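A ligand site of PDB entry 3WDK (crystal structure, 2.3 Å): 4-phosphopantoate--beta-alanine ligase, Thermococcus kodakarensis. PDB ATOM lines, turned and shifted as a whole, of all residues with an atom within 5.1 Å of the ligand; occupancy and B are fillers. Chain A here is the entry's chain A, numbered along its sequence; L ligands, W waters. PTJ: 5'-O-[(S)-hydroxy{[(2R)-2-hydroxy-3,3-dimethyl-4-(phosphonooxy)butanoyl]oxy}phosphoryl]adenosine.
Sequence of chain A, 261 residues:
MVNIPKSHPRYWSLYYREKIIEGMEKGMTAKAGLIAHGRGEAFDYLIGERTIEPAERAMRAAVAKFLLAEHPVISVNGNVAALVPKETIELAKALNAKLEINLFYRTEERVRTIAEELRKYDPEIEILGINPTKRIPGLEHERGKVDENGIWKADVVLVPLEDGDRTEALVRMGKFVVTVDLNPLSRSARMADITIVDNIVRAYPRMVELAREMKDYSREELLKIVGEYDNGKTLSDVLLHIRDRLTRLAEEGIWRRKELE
O of Gly 33 is in hydrogen-bond range of ND2 of Asn 79 (3.1 Å).
ND2 of Asn 77 lies within hydrogen-bond range of O of Leu 161, 3.3 Å away.
The backbone carbonyl oxygen (O) of Val 180 is in hydrogen-bond range of the backbone NH (N) of Leu 161.
The side-chain carboxylate (OD2) of Asp 181 is in hydrogen-bond range of the side-chain hydroxyl (OG) of Ser 186 (3.4 Å).
The backbone carbonyl oxygen (O) of Tyr 105 lies within hydrogen-bond range of the guanidinium group (NH1) of Arg 110, 2.8 Å away.
OD1 of Asn 77 lies within hydrogen-bond range of N of Asn 79, 2.8 Å away.
O of Asn 183 sits at hydrogen-bond distance from OG of Ser 186, 2.9 Å away.
The backbone NH of Asn 183 is in hydrogen-bond range of the side-chain carboxylate of Asp 181, at 2.9 Å.
The side-chain carboxylate of Asp 181 sits at hydrogen-bond distance from an oxygen (O3') of the ligand, at 2.5 Å.
The backbone carbonyl oxygen of Leu 161 sits at hydrogen-bond distance from an oxygen (O13) of the ligand (2.7 Å).
A nitrogen (N1) of the ligand sits at hydrogen-bond distance from the backbone NH (N) of Ile 200.
A nitrogen (N3) of the ligand sits at hydrogen-bond distance from the backbone NH (N) of Leu 182, at 3.1 Å.
The backbone NH (N) of Phe 104 is in hydrogen-bond range of an oxygen (O16) of the ligand (2.7 Å).
The guanidinium group (NH1) of Arg 110 lies within salt-bridge range of an oxygen (O15) of the ligand.
The backbone NH (N) of Gly 40 is in hydrogen-bond range of an oxygen (O2') of the ligand, at 3.5 Å.
The backbone NH (N) of Tyr 105 lies within hydrogen-bond range of an oxygen (O15) of the ligand (2.9 Å).
A nitrogen (N6) of the ligand sits close to the side-chain amide nitrogen (ND2) of Asn 199.
An oxygen (O17) of the ligand lies within hydrogen-bond range of the backbone NH of Gly 78 (2.9 Å).
Water W5 lies within hydrogen-bond range of an oxygen (O16) of the ligand (2.8 Å), the side-chain carboxylate of Glu 162 (3.1 Å) and the side-chain amide nitrogen of Asn 77 (3.4 Å).
Water W3 lies within hydrogen-bond range of an oxygen (O2') of the ligand (2.8 Å) and the side-chain amide nitrogen (ND2) of Asn 183 (3.0 Å).
Water W2 lies within hydrogen-bond range of an oxygen (O17) of the ligand (2.9 Å), the backbone NH of Ala 30 (2.9 Å), the side-chain amide oxygen of Asn 79 (3.0 Å) and the guanidinium group of Arg 110 (3.1 Å).
Water W1 lies within hydrogen-bond range of ND1 of His 37 (2.9 Å), ND2 of Asn 79 (2.9 Å) and N7 of the ligand (3.0 Å).
Water W6 bridges N of Gly 164 and O1P of the ligand.
Water W4 bridges the backbone carbonyl oxygen of His 37 (2.9 Å) and a nitrogen (N6) of the ligand (3.2 Å).
Merely in contact with the ligand: Asp 198, Ala 36, Leu 103, Asn 77, Asn 183, Asp 163, Glu 162, Gly 33, Ala 32, Asn 79 and Arg 39.
Hydrophobic or aromatic side chains within 4 Å of the ligand: Ala 32, Ala 36, Leu 103, Phe 104, Tyr 105, Leu 161, Leu 182 and Ile 200.
21 residues have an atom within 4 Å of the ligand: Ala 32, Gly 33, Ala 36, Arg 39, Gly 40, Asn 77, Gly 78, Asn 79, Leu 103, Phe 104, Tyr 105, Arg 110, Leu 161, Glu 162, Asp 163, Asp 181, Leu 182, Asn 183, Asp 198, Asn 199 and Ile 200.
The nearest printed residue that does not touch the ligand is Asn 102 (4.02 Å).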
ATOM      1  N   ALA A  30       0.067 -28.854 -14.593  1.00  0.00           N
ATOM      2  CA  ALA A  30      -1.336 -29.232 -14.565  1.00  0.00           C
ATOM      3  C   ALA A  30      -2.004 -28.930 -15.908  1.00  0.00           C
ATOM      4  O   ALA A  30      -1.471 -28.145 -16.698  1.00  0.00           O
ATOM      5  CB  ALA A  30      -2.039 -28.481 -13.463  1.00  0.00           C
ATOM      6  N   ALA A  32      -4.686 -27.344 -16.248  1.00  0.00           N
ATOM      7  CA  ALA A  32      -5.108 -25.966 -16.094  1.00  0.00           C
ATOM      8  C   ALA A  32      -3.944 -25.093 -16.540  1.00  0.00           C
ATOM      9  O   ALA A  32      -4.137 -23.958 -16.977  1.00  0.00           O
ATOM     10  CB  ALA A  32      -5.451 -25.679 -14.648  1.00  0.00           C
ATOM     11  N   GLY A  33      -2.736 -25.622 -16.407  1.00  0.00           N
ATOM     12  CA  GLY A  33      -1.549 -24.895 -16.794  1.00  0.00           C
ATOM     13  C   GLY A  33      -1.450 -24.704 -18.296  1.00  0.00           C
ATOM     14  O   GLY A  33      -0.917 -23.696 -18.767  1.00  0.00           O
ATOM     15  N   ALA A  36      -3.824 -21.953 -19.001  1.00  0.00           N
ATOM     16  CA  ALA A  36      -3.196 -20.708 -18.576  1.00  0.00           C
ATOM     17  C   ALA A  36      -2.161 -20.227 -19.581  1.00  0.00           C
ATOM     18  O   ALA A  36      -2.122 -19.043 -19.919  1.00  0.00           O
ATOM     19  CB  ALA A  36      -2.546 -20.898 -17.204  1.00  0.00           C
ATOM     20  N   HIS A  37      -1.329 -21.146 -20.067  1.00  0.00           N
ATOM     21  CA  HIS A  37      -0.295 -20.793 -21.030  1.00  0.00           C
ATOM     22  C   HIS A  37      -0.917 -20.164 -22.271  1.00  0.00           C
ATOM     23  O   HIS A  37      -0.378 -19.205 -22.829  1.00  0.00           O
ATOM     24  CB  HIS A  37       0.497 -22.034 -21.441  1.00  0.00           C
ATOM     25  CG  HIS A  37       1.701 -21.720 -22.274  1.00  0.00           C
ATOM     26  ND1 HIS A  37       2.887 -21.286 -21.730  1.00  0.00           N
ATOM     27  CD2 HIS A  37       1.869 -21.709 -23.619  1.00  0.00           C
ATOM     28  CE1 HIS A  37       3.740 -21.014 -22.712  1.00  0.00           C
ATOM     29  NE2 HIS A  37       3.146 -21.264 -23.859  1.00  0.00           N
ATOM     30  N   ARG A  39      -3.840 -18.565 -22.499  1.00  0.00           N
ATOM     31  CA  ARG A  39      -4.349 -17.242 -22.181  1.00  0.00           C
ATOM     32  C   ARG A  39      -3.189 -16.248 -22.222  1.00  0.00           C
ATOM     33  O   ARG A  39      -3.319 -15.148 -22.766  1.00  0.00           O
ATOM     34  CB  ARG A  39      -4.960 -17.237 -20.788  1.00  0.00           C
ATOM     35  CG  ARG A  39      -6.176 -18.136 -20.658  1.00  0.00           C
ATOM     36  CD  ARG A  39      -6.818 -18.012 -19.268  1.00  0.00           C
ATOM     37  NE  ARG A  39      -8.196 -18.467 -19.289  1.00  0.00           N
ATOM     38  CZ  ARG A  39      -9.130 -18.074 -18.429  1.00  0.00           C
ATOM     39  NH1 ARG A  39     -10.369 -18.548 -18.541  1.00  0.00           N
ATOM     40  NH2 ARG A  39      -8.839 -17.216 -17.456  1.00  0.00           N
ATOM     41  N   GLY A  40      -2.048 -16.640 -21.657  1.00  0.00           N
ATOM     42  CA  GLY A  40      -0.897 -15.769 -21.651  1.00  0.00           C
ATOM     43  C   GLY A  40      -0.463 -15.420 -23.070  1.00  0.00           C
ATOM     44  O   GLY A  40      -0.068 -14.292 -23.350  1.00  0.00           O
ATOM     45  N   PHE A  43      -2.473 -12.592 -24.560  1.00  0.00           N
ATOM     46  CA  PHE A  43      -2.018 -11.308 -24.080  1.00  0.00           C
ATOM     47  C   PHE A  43      -0.625 -10.966 -24.593  1.00  0.00           C
ATOM     48  O   PHE A  43      -0.290  -9.792 -24.746  1.00  0.00           O
ATOM     49  CB  PHE A  43      -2.102 -11.265 -22.571  1.00  0.00           C
ATOM     50  CG  PHE A  43      -3.487 -11.041 -22.059  1.00  0.00           C
ATOM     51  CD1 PHE A  43      -4.039  -9.771 -22.039  1.00  0.00           C
ATOM     52  CD2 PHE A  43      -4.278 -12.119 -21.673  1.00  0.00           C
ATOM     53  CE1 PHE A  43      -5.343  -9.558 -21.644  1.00  0.00           C
ATOM     54  CE2 PHE A  43      -5.600 -11.923 -21.273  1.00  0.00           C
ATOM     55  CZ  PHE A  43      -6.135 -10.636 -21.259  1.00  0.00           C
ATOM     56  N   ASN A  77       5.703 -22.790  -9.585  1.00  0.00           N
ATOM     57  CA  ASN A  77       4.537 -23.618  -9.871  1.00  0.00           C
ATOM     58  C   ASN A  77       4.814 -24.498 -11.095  1.00  0.00           C
ATOM     59  O   ASN A  77       5.899 -24.452 -11.678  1.00  0.00           O
ATOM     60  CB  ASN A  77       3.279 -22.775 -10.102  1.00  0.00           C
ATOM     61  CG  ASN A  77       3.379 -21.849 -11.321  1.00  0.00           C
ATOM     62  OD1 ASN A  77       4.063 -22.148 -12.303  1.00  0.00           O
ATOM     63  ND2 ASN A  77       2.677 -20.721 -11.251  1.00  0.00           N
ATOM     64  N   GLY A  78       3.827 -25.307 -11.478  1.00  0.00           N
ATOM     65  CA  GLY A  78       3.990 -26.173 -12.628  1.00  0.00           C
ATOM     66  C   GLY A  78       4.419 -25.483 -13.915  1.00  0.00           C
ATOM     67  O   GLY A  78       5.194 -26.045 -14.693  1.00  0.00           O
ATOM     68  N   ASN A  79       3.904 -24.278 -14.166  1.00  0.00           N
ATOM     69  CA  ASN A  79       4.245 -23.560 -15.390  1.00  0.00           C
ATOM     70  C   ASN A  79       5.672 -23.030 -15.344  1.00  0.00           C
ATOM     71  O   ASN A  79       6.386 -23.057 -16.346  1.00  0.00           O
ATOM     72  CB  ASN A  79       3.258 -22.414 -15.631  1.00  0.00           C
ATOM     73  CG  ASN A  79       1.920 -22.902 -16.135  1.00  0.00           C
ATOM     74  OD1 ASN A  79       1.309 -23.793 -15.542  1.00  0.00           O
ATOM     75  ND2 ASN A  79       1.451 -22.330 -17.240  1.00  0.00           N
ATOM     76  N   LEU A  83       8.821 -23.933 -17.898  1.00  0.00           N
ATOM     77  CA  LEU A  83       9.372 -22.867 -18.718  1.00  0.00           C
ATOM     78  C   LEU A  83      10.738 -22.306 -18.343  1.00  0.00           C
ATOM     79  O   LEU A  83      11.611 -22.137 -19.192  1.00  0.00           O
ATOM     80  CB  LEU A  83       8.369 -21.713 -18.783  1.00  0.00           C
ATOM     81  CG  LEU A  83       7.004 -22.045 -19.411  1.00  0.00           C
ATOM     82  CD1 LEU A  83       6.051 -20.892 -19.212  1.00  0.00           C
ATOM     83  CD2 LEU A  83       7.194 -22.359 -20.893  1.00  0.00           C
ATOM     84  N   ASN A 102       5.083 -23.972  -4.680  1.00  0.00           N
ATOM     85  CA  ASN A 102       3.748 -23.705  -4.157  1.00  0.00           C
ATOM     86  C   ASN A 102       2.758 -23.814  -5.303  1.00  0.00           C
ATOM     87  O   ASN A 102       2.693 -22.951  -6.169  1.00  0.00           O
ATOM     88  CB  ASN A 102       3.686 -22.321  -3.520  1.00  0.00           C
ATOM     89  CG  ASN A 102       2.319 -22.019  -2.924  1.00  0.00           C
ATOM     90  OD1 ASN A 102       1.388 -21.634  -3.621  1.00  0.00           O
ATOM     91  ND2 ASN A 102       2.195 -22.216  -1.610  1.00  0.00           N
ATOM     92  N   LEU A 103       1.988 -24.906  -5.290  1.00  0.00           N
ATOM     93  CA  LEU A 103       1.009 -25.180  -6.335  1.00  0.00           C
ATOM     94  C   LEU A 103      -0.417 -24.822  -5.928  1.00  0.00           C
ATOM     95  O   LEU A 103      -0.805 -24.991  -4.775  1.00  0.00           O
ATOM     96  CB  LEU A 103       1.079 -26.660  -6.702  1.00  0.00           C
ATOM     97  CG  LEU A 103       2.230 -27.147  -7.598  1.00  0.00           C
ATOM     98  CD1 LEU A 103       3.416 -26.206  -7.517  1.00  0.00           C
ATOM     99  CD2 LEU A 103       2.622 -28.563  -7.183  1.00  0.00           C
ATOM    100  N   PHE A 104      -1.187 -24.340  -6.898  1.00  0.00           N
ATOM    101  CA  PHE A 104      -2.582 -23.983  -6.670  1.00  0.00           C
ATOM    102  C   PHE A 104      -3.419 -25.258  -6.739  1.00  0.00           C
ATOM    103  O   PHE A 104      -4.396 -25.424  -6.001  1.00  0.00           O
ATOM    104  CB  PHE A 104      -3.038 -22.968  -7.725  1.00  0.00           C
ATOM    105  CG  PHE A 104      -4.445 -22.481  -7.518  1.00  0.00           C
ATOM    106  CD1 PHE A 104      -5.521 -23.162  -8.074  1.00  0.00           C
ATOM    107  CD2 PHE A 104      -4.691 -21.326  -6.770  1.00  0.00           C
ATOM    108  CE1 PHE A 104      -6.824 -22.708  -7.873  1.00  0.00           C
ATOM    109  CE2 PHE A 104      -5.989 -20.870  -6.562  1.00  0.00           C
ATOM    110  CZ  PHE A 104      -7.058 -21.562  -7.117  1.00  0.00           C
ATOM    111  N   TYR A 105      -3.035 -26.155  -7.643  1.00  0.00           N
ATOM    112  CA  TYR A 105      -3.688 -27.449  -7.809  1.00  0.00           C
ATOM    113  C   TYR A 105      -2.648 -28.461  -7.351  1.00  0.00           C
ATOM    114  O   TYR A 105      -2.189 -29.303  -8.111  1.00  0.00           O
ATOM    115  CB  TYR A 105      -4.039 -27.690  -9.275  1.00  0.00           C
ATOM    116  CG  TYR A 105      -5.046 -26.721  -9.843  1.00  0.00           C
ATOM    117  CD1 TYR A 105      -6.385 -26.750  -9.437  1.00  0.00           C
ATOM    118  CD2 TYR A 105      -4.665 -25.760 -10.782  1.00  0.00           C
ATOM    119  CE1 TYR A 105      -7.319 -25.861  -9.957  1.00  0.00           C
ATOM    120  CE2 TYR A 105      -5.592 -24.859 -11.300  1.00  0.00           C
ATOM    121  CZ  TYR A 105      -6.912 -24.910 -10.885  1.00  0.00           C
ATOM    122  OH  TYR A 105      -7.823 -24.017 -11.411  1.00  0.00           O
ATOM    123  N   ARG A 106      -2.284 -28.359  -6.068  1.00  0.00           N
ATOM    124  CA  ARG A 106      -1.265 -29.199  -5.474  1.00  0.00           C
ATOM    125  C   ARG A 106      -1.580 -30.661  -5.185  1.00  0.00           C
ATOM    126  O   ARG A 106      -2.688 -31.017  -4.792  1.00  0.00           O
ATOM    127  CB  ARG A 106      -0.766 -28.560  -4.179  1.00  0.00           C
ATOM    128  CG  ARG A 106       0.193 -29.438  -3.382  1.00  0.00           C
ATOM    129  CD  ARG A 106       0.808 -28.725  -2.189  1.00  0.00           C
ATOM    130  NE  ARG A 106       1.751 -29.602  -1.498  1.00  0.00           N
ATOM    131  CZ  ARG A 106       2.828 -29.181  -0.845  1.00  0.00           C
ATOM    132  NH1 ARG A 106       3.627 -30.050  -0.251  1.00  0.00           N
ATOM    133  NH2 ARG A 106       3.121 -27.884  -0.814  1.00  0.00           N
ATOM    134  N   ARG A 110       3.288 -33.948  -7.817  1.00  0.00           N
ATOM    135  CA  ARG A 110       3.649 -32.826  -8.681  1.00  0.00           C
ATOM    136  C   ARG A 110       4.810 -32.079  -8.019  1.00  0.00           C
ATOM    137  O   ARG A 110       5.777 -31.699  -8.687  1.00  0.00           O
ATOM    138  CB  ARG A 110       2.472 -31.858  -8.867  1.00  0.00           C
ATOM    139  CG  ARG A 110       1.329 -32.388  -9.738  1.00  0.00           C
ATOM    140  CD  ARG A 110       0.374 -31.245 -10.079  1.00  0.00           C
ATOM    141  NE  ARG A 110       1.095 -30.161 -10.728  1.00  0.00           N
ATOM    142  CZ  ARG A 110       0.732 -28.878 -10.705  1.00  0.00           C
ATOM    143  NH1 ARG A 110      -0.373 -28.507 -10.065  1.00  0.00           N
ATOM    144  NH2 ARG A 110       1.474 -27.966 -11.322  1.00  0.00           N
ATOM    145  N   LEU A 161       2.538 -16.105 -12.496  1.00  0.00           N
ATOM    146  CA  LEU A 161       1.452 -16.849 -13.108  1.00  0.00           C
ATOM    147  C   LEU A 161       0.572 -17.435 -12.012  1.00  0.00           C
ATOM    148  O   LEU A 161       0.264 -18.634 -11.997  1.00  0.00           O
ATOM    149  CB  LEU A 161       2.033 -17.952 -13.986  1.00  0.00           C
ATOM    150  CG  LEU A 161       2.629 -17.554 -15.346  1.00  0.00           C
ATOM    151  CD1 LEU A 161       3.723 -16.515 -15.202  1.00  0.00           C
ATOM    152  CD2 LEU A 161       3.160 -18.802 -16.022  1.00  0.00           C
ATOM    153  N   GLU A 162       0.156 -16.564 -11.100  1.00  0.00           N
ATOM    154  CA  GLU A 162      -0.653 -16.958  -9.968  1.00  0.00           C
ATOM    155  C   GLU A 162      -2.139 -16.674 -10.111  1.00  0.00           C
ATOM    156  O   GLU A 162      -2.547 -15.729 -10.796  1.00  0.00           O
ATOM    157  CB  GLU A 162      -0.143 -16.257  -8.707  1.00  0.00           C
ATOM    158  CG  GLU A 162      -0.860 -16.717  -7.456  1.00  0.00           C
ATOM    159  CD  GLU A 162      -0.607 -18.189  -7.165  1.00  0.00           C
ATOM    160  OE1 GLU A 162       0.488 -18.502  -6.641  1.00  0.00           O
ATOM    161  OE2 GLU A 162      -1.491 -19.019  -7.469  1.00  0.00           O
ATOM    162  N   ASP A 163      -2.947 -17.491  -9.449  1.00  0.00           N
ATOM    163  CA  ASP A 163      -4.385 -17.311  -9.451  1.00  0.00           C
ATOM    164  C   ASP A 163      -4.676 -16.049  -8.652  1.00  0.00           C
ATOM    165  O   ASP A 163      -4.093 -15.841  -7.584  1.00  0.00           O
ATOM    166  CB  ASP A 163      -5.075 -18.514  -8.799  1.00  0.00           C
ATOM    167  CG  ASP A 163      -6.580 -18.342  -8.712  1.00  0.00           C
ATOM    168  OD1 ASP A 163      -7.040 -17.546  -7.867  1.00  0.00           O
ATOM    169  OD2 ASP A 163      -7.293 -18.993  -9.512  1.00  0.00           O
ATOM    170  N   GLY A 164      -5.580 -15.216  -9.157  1.00  0.00           N
ATOM    171  CA  GLY A 164      -5.913 -13.982  -8.485  1.00  0.00           C
ATOM    172  C   GLY A 164      -6.187 -14.066  -6.995  1.00  0.00           C
ATOM    173  O   GLY A 164      -5.626 -13.305  -6.211  1.00  0.00           O
ATOM    174  N   VAL A 180       4.407 -11.797 -12.010  1.00  0.00           N
ATOM    175  CA  VAL A 180       4.698 -11.708 -13.423  1.00  0.00           C
ATOM    176  C   VAL A 180       3.411 -12.223 -14.042  1.00  0.00           C
ATOM    177  O   VAL A 180       3.028 -13.379 -13.810  1.00  0.00           O
ATOM    178  CB  VAL A 180       5.872 -12.617 -13.819  1.00  0.00           C
ATOM    179  CG1 VAL A 180       6.089 -12.588 -15.322  1.00  0.00           C
ATOM    180  CG2 VAL A 180       7.138 -12.156 -13.096  1.00  0.00           C
ATOM    181  N   ASP A 181       2.743 -11.381 -14.809  1.00  0.00           N
ATOM    182  CA  ASP A 181       1.480 -11.754 -15.415  1.00  0.00           C
ATOM    183  C   ASP A 181       1.210 -10.980 -16.696  1.00  0.00           C
ATOM    184  O   ASP A 181       1.133  -9.745 -16.687  1.00  0.00           O
ATOM    185  CB  ASP A 181       0.351 -11.515 -14.416  1.00  0.00           C
ATOM    186  CG  ASP A 181      -0.876 -12.352 -14.720  1.00  0.00           C
ATOM    187  OD1 ASP A 181      -1.271 -12.401 -15.898  1.00  0.00           O
ATOM    188  OD2 ASP A 181      -1.433 -12.941 -13.774  1.00  0.00           O
ATOM    189  N   LEU A 182       1.044 -11.697 -17.792  1.00  0.00           N
ATOM    190  CA  LEU A 182       0.785 -11.070 -19.083  1.00  0.00           C
ATOM    191  C   LEU A 182      -0.597 -10.415 -19.171  1.00  0.00           C
ATOM    192  O   LEU A 182      -0.832  -9.579 -20.036  1.00  0.00           O
ATOM    193  CB  LEU A 182       0.980 -12.102 -20.210  1.00  0.00           C
ATOM    194  CG  LEU A 182       2.447 -12.317 -20.616  1.00  0.00           C
ATOM    195  CD1 LEU A 182       2.667 -13.690 -21.265  1.00  0.00           C
ATOM    196  CD2 LEU A 182       2.858 -11.204 -21.564  1.00  0.00           C
ATOM    197  N   ASN A 183      -1.499 -10.782 -18.271  1.00  0.00           N
ATOM    198  CA  ASN A 183      -2.850 -10.195 -18.262  1.00  0.00           C
ATOM    199  C   ASN A 183      -2.887  -9.037 -17.274  1.00  0.00           C
ATOM    200  O   ASN A 183      -3.052  -9.236 -16.059  1.00  0.00           O
ATOM    201  CB  ASN A 183      -3.880 -11.254 -17.858  1.00  0.00           C
ATOM    202  CG  ASN A 183      -5.316 -10.749 -17.962  1.00  0.00           C
ATOM    203  OD1 ASN A 183      -5.576  -9.541 -17.979  1.00  0.00           O
ATOM    204  ND2 ASN A 183      -6.243 -11.680 -18.023  1.00  0.00           N
ATOM    205  N   SER A 186      -6.039  -8.950 -14.980  1.00  0.00           N
ATOM    206  CA  SER A 186      -6.328 -10.038 -14.052  1.00  0.00           C
ATOM    207  C   SER A 186      -6.363  -9.564 -12.606  1.00  0.00           C
ATOM    208  O   SER A 186      -5.794  -8.530 -12.269  1.00  0.00           O
ATOM    209  CB  SER A 186      -5.265 -11.138 -14.183  1.00  0.00           C
ATOM    210  OG  SER A 186      -3.994 -10.672 -13.740  1.00  0.00           O
ATOM    211  N   ASP A 198       4.871  -9.127 -18.646  1.00  0.00           N
ATOM    212  CA  ASP A 198       5.838  -9.588 -19.617  1.00  0.00           C
ATOM    213  C   ASP A 198       5.791 -11.108 -19.533  1.00  0.00           C
ATOM    214  O   ASP A 198       5.306 -11.666 -18.548  1.00  0.00           O
ATOM    215  CB  ASP A 198       7.223  -9.070 -19.211  1.00  0.00           C
ATOM    216  CG  ASP A 198       8.238  -9.128 -20.337  1.00  0.00           C
ATOM    217  OD1 ASP A 198       7.896  -9.563 -21.441  1.00  0.00           O
ATOM    218  OD2 ASP A 198       9.390  -8.727 -20.092  1.00  0.00           O
ATOM    219  N   ASN A 199       6.263 -11.796 -20.575  1.00  0.00           N
ATOM    220  CA  ASN A 199       6.260 -13.249 -20.565  1.00  0.00           C
ATOM    221  C   ASN A 199       7.367 -13.647 -19.584  1.00  0.00           C
ATOM    222  O   ASN A 199       8.493 -13.138 -19.654  1.00  0.00           O
ATOM    223  CB  ASN A 199       6.566 -13.793 -21.966  1.00  0.00           C
ATOM    224  CG  ASN A 199       6.218 -15.278 -22.125  1.00  0.00           C
ATOM    225  OD1 ASN A 199       5.479 -15.651 -23.038  1.00  0.00           O
ATOM    226  ND2 ASN A 199       6.749 -16.116 -21.249  1.00  0.00           N
ATOM    227  N   ILE A 200       7.054 -14.557 -18.676  1.00  0.00           N
ATOM    228  CA  ILE A 200       8.051 -14.982 -17.697  1.00  0.00           C
ATOM    229  C   ILE A 200       9.366 -15.418 -18.342  1.00  0.00           C
ATOM    230  O   ILE A 200      10.427 -15.202 -17.772  1.00  0.00           O
ATOM    231  CB  ILE A 200       7.525 -16.136 -16.818  1.00  0.00           C
ATOM    232  CG1 ILE A 200       8.434 -16.308 -15.599  1.00  0.00           C
ATOM    233  CG2 ILE A 200       7.467 -17.432 -17.627  1.00  0.00           C
ATOM    234  CD1 ILE A 200       7.918 -17.296 -14.565  1.00  0.00           C
HETATM  235  O15 PTJ L   1      -1.037 -25.921  -9.799  1.00  0.00           O
HETATM  236  P1  PTJ L   1      -0.166 -24.820 -10.263  1.00  0.00           P
HETATM  237  O16 PTJ L   1       0.216 -23.861  -9.203  1.00  0.00           O
HETATM  238  O17 PTJ L   1       0.957 -25.249 -11.125  1.00  0.00           O
HETATM  239  O14 PTJ L   1      -1.123 -23.974 -11.242  1.00  0.00           O
HETATM  240  C16 PTJ L   1      -0.570 -23.083 -12.210  1.00  0.00           C
HETATM  241  C13 PTJ L   1      -1.688 -22.249 -12.848  1.00  0.00           C
HETATM  242  C14 PTJ L   1      -1.069 -21.293 -13.864  1.00  0.00           C
HETATM  243  C15 PTJ L   1      -2.678 -23.179 -13.554  1.00  0.00           C
HETATM  244  C12 PTJ L   1      -2.415 -21.455 -11.761  1.00  0.00           C
HETATM  245  O13 PTJ L   1      -1.494 -20.557 -11.136  1.00  0.00           O
HETATM  246  C11 PTJ L   1      -3.571 -20.656 -12.370  1.00  0.00           C
HETATM  247  O12 PTJ L   1      -4.735 -21.056 -12.283  1.00  0.00           O
HETATM  248  O11 PTJ L   1      -3.225 -19.454 -12.908  1.00  0.00           O
HETATM  249  P   PTJ L   1      -4.302 -18.514 -13.634  1.00  0.00           P
HETATM  250  O1P PTJ L   1      -5.386 -18.181 -12.681  1.00  0.00           O
HETATM  251  O2P PTJ L   1      -4.660 -19.136 -14.933  1.00  0.00           O
HETATM  252  O5' PTJ L   1      -3.443 -17.188 -13.926  1.00  0.00           O
HETATM  253  C5' PTJ L   1      -2.207 -17.300 -14.640  1.00  0.00           C
HETATM  254  C4' PTJ L   1      -1.828 -15.931 -15.220  1.00  0.00           C
HETATM  255  O4' PTJ L   1      -0.543 -16.085 -15.847  1.00  0.00           O
HETATM  256  C3' PTJ L   1      -2.806 -15.533 -16.305  1.00  0.00           C
HETATM  257  O3' PTJ L   1      -3.064 -14.119 -16.243  1.00  0.00           O
HETATM  258  C2' PTJ L   1      -2.064 -15.879 -17.581  1.00  0.00           C
HETATM  259  O2' PTJ L   1      -2.457 -14.982 -18.619  1.00  0.00           O
HETATM  260  C1' PTJ L   1      -0.653 -15.532 -17.160  1.00  0.00           C
HETATM  261  N9  PTJ L   1       0.384 -16.112 -18.052  1.00  0.00           N
HETATM  262  C8  PTJ L   1       0.294 -17.310 -18.634  1.00  0.00           C
HETATM  263  N7  PTJ L   1       1.504 -17.617 -19.103  1.00  0.00           N
HETATM  264  C5  PTJ L   1       2.327 -16.603 -18.822  1.00  0.00           C
HETATM  265  C4  PTJ L   1       1.634 -15.683 -18.163  1.00  0.00           C
HETATM  266  N3  PTJ L   1       2.219 -14.542 -17.752  1.00  0.00           N
HETATM  267  C2  PTJ L   1       3.572 -14.323 -18.041  1.00  0.00           C
HETATM  268  N1  PTJ L   1       4.259 -15.313 -18.744  1.00  0.00           N
HETATM  269  C6  PTJ L   1       3.614 -16.420 -19.113  1.00  0.00           C
HETATM  270  N6  PTJ L   1       4.189 -17.345 -19.880  1.00  0.00           N
HETATM  271  O   HOH W   1       2.584 -20.390 -19.027  1.00  0.00           O
HETATM  272  O   HOH W   2       1.074 -26.204 -13.828  1.00  0.00           O
HETATM  273  O   HOH W   3      -5.240 -14.485 -18.450  1.00  0.00           O
HETATM  274  O   HOH W   4       2.123 -17.854 -22.287  1.00  0.00           O
HETATM  275  O   HOH W   5       0.368 -21.133  -8.850  1.00  0.00           O
HETATM  276  O   HOH W   6      -6.724 -15.615 -11.836  1.00  0.00           O
HETATM  277  O   HOH W   7      -3.690 -14.445 -13.010  1.00  0.00           O
HETATM  278  O   HOH W   8      -6.932 -21.497 -15.507  1.00  0.00           O
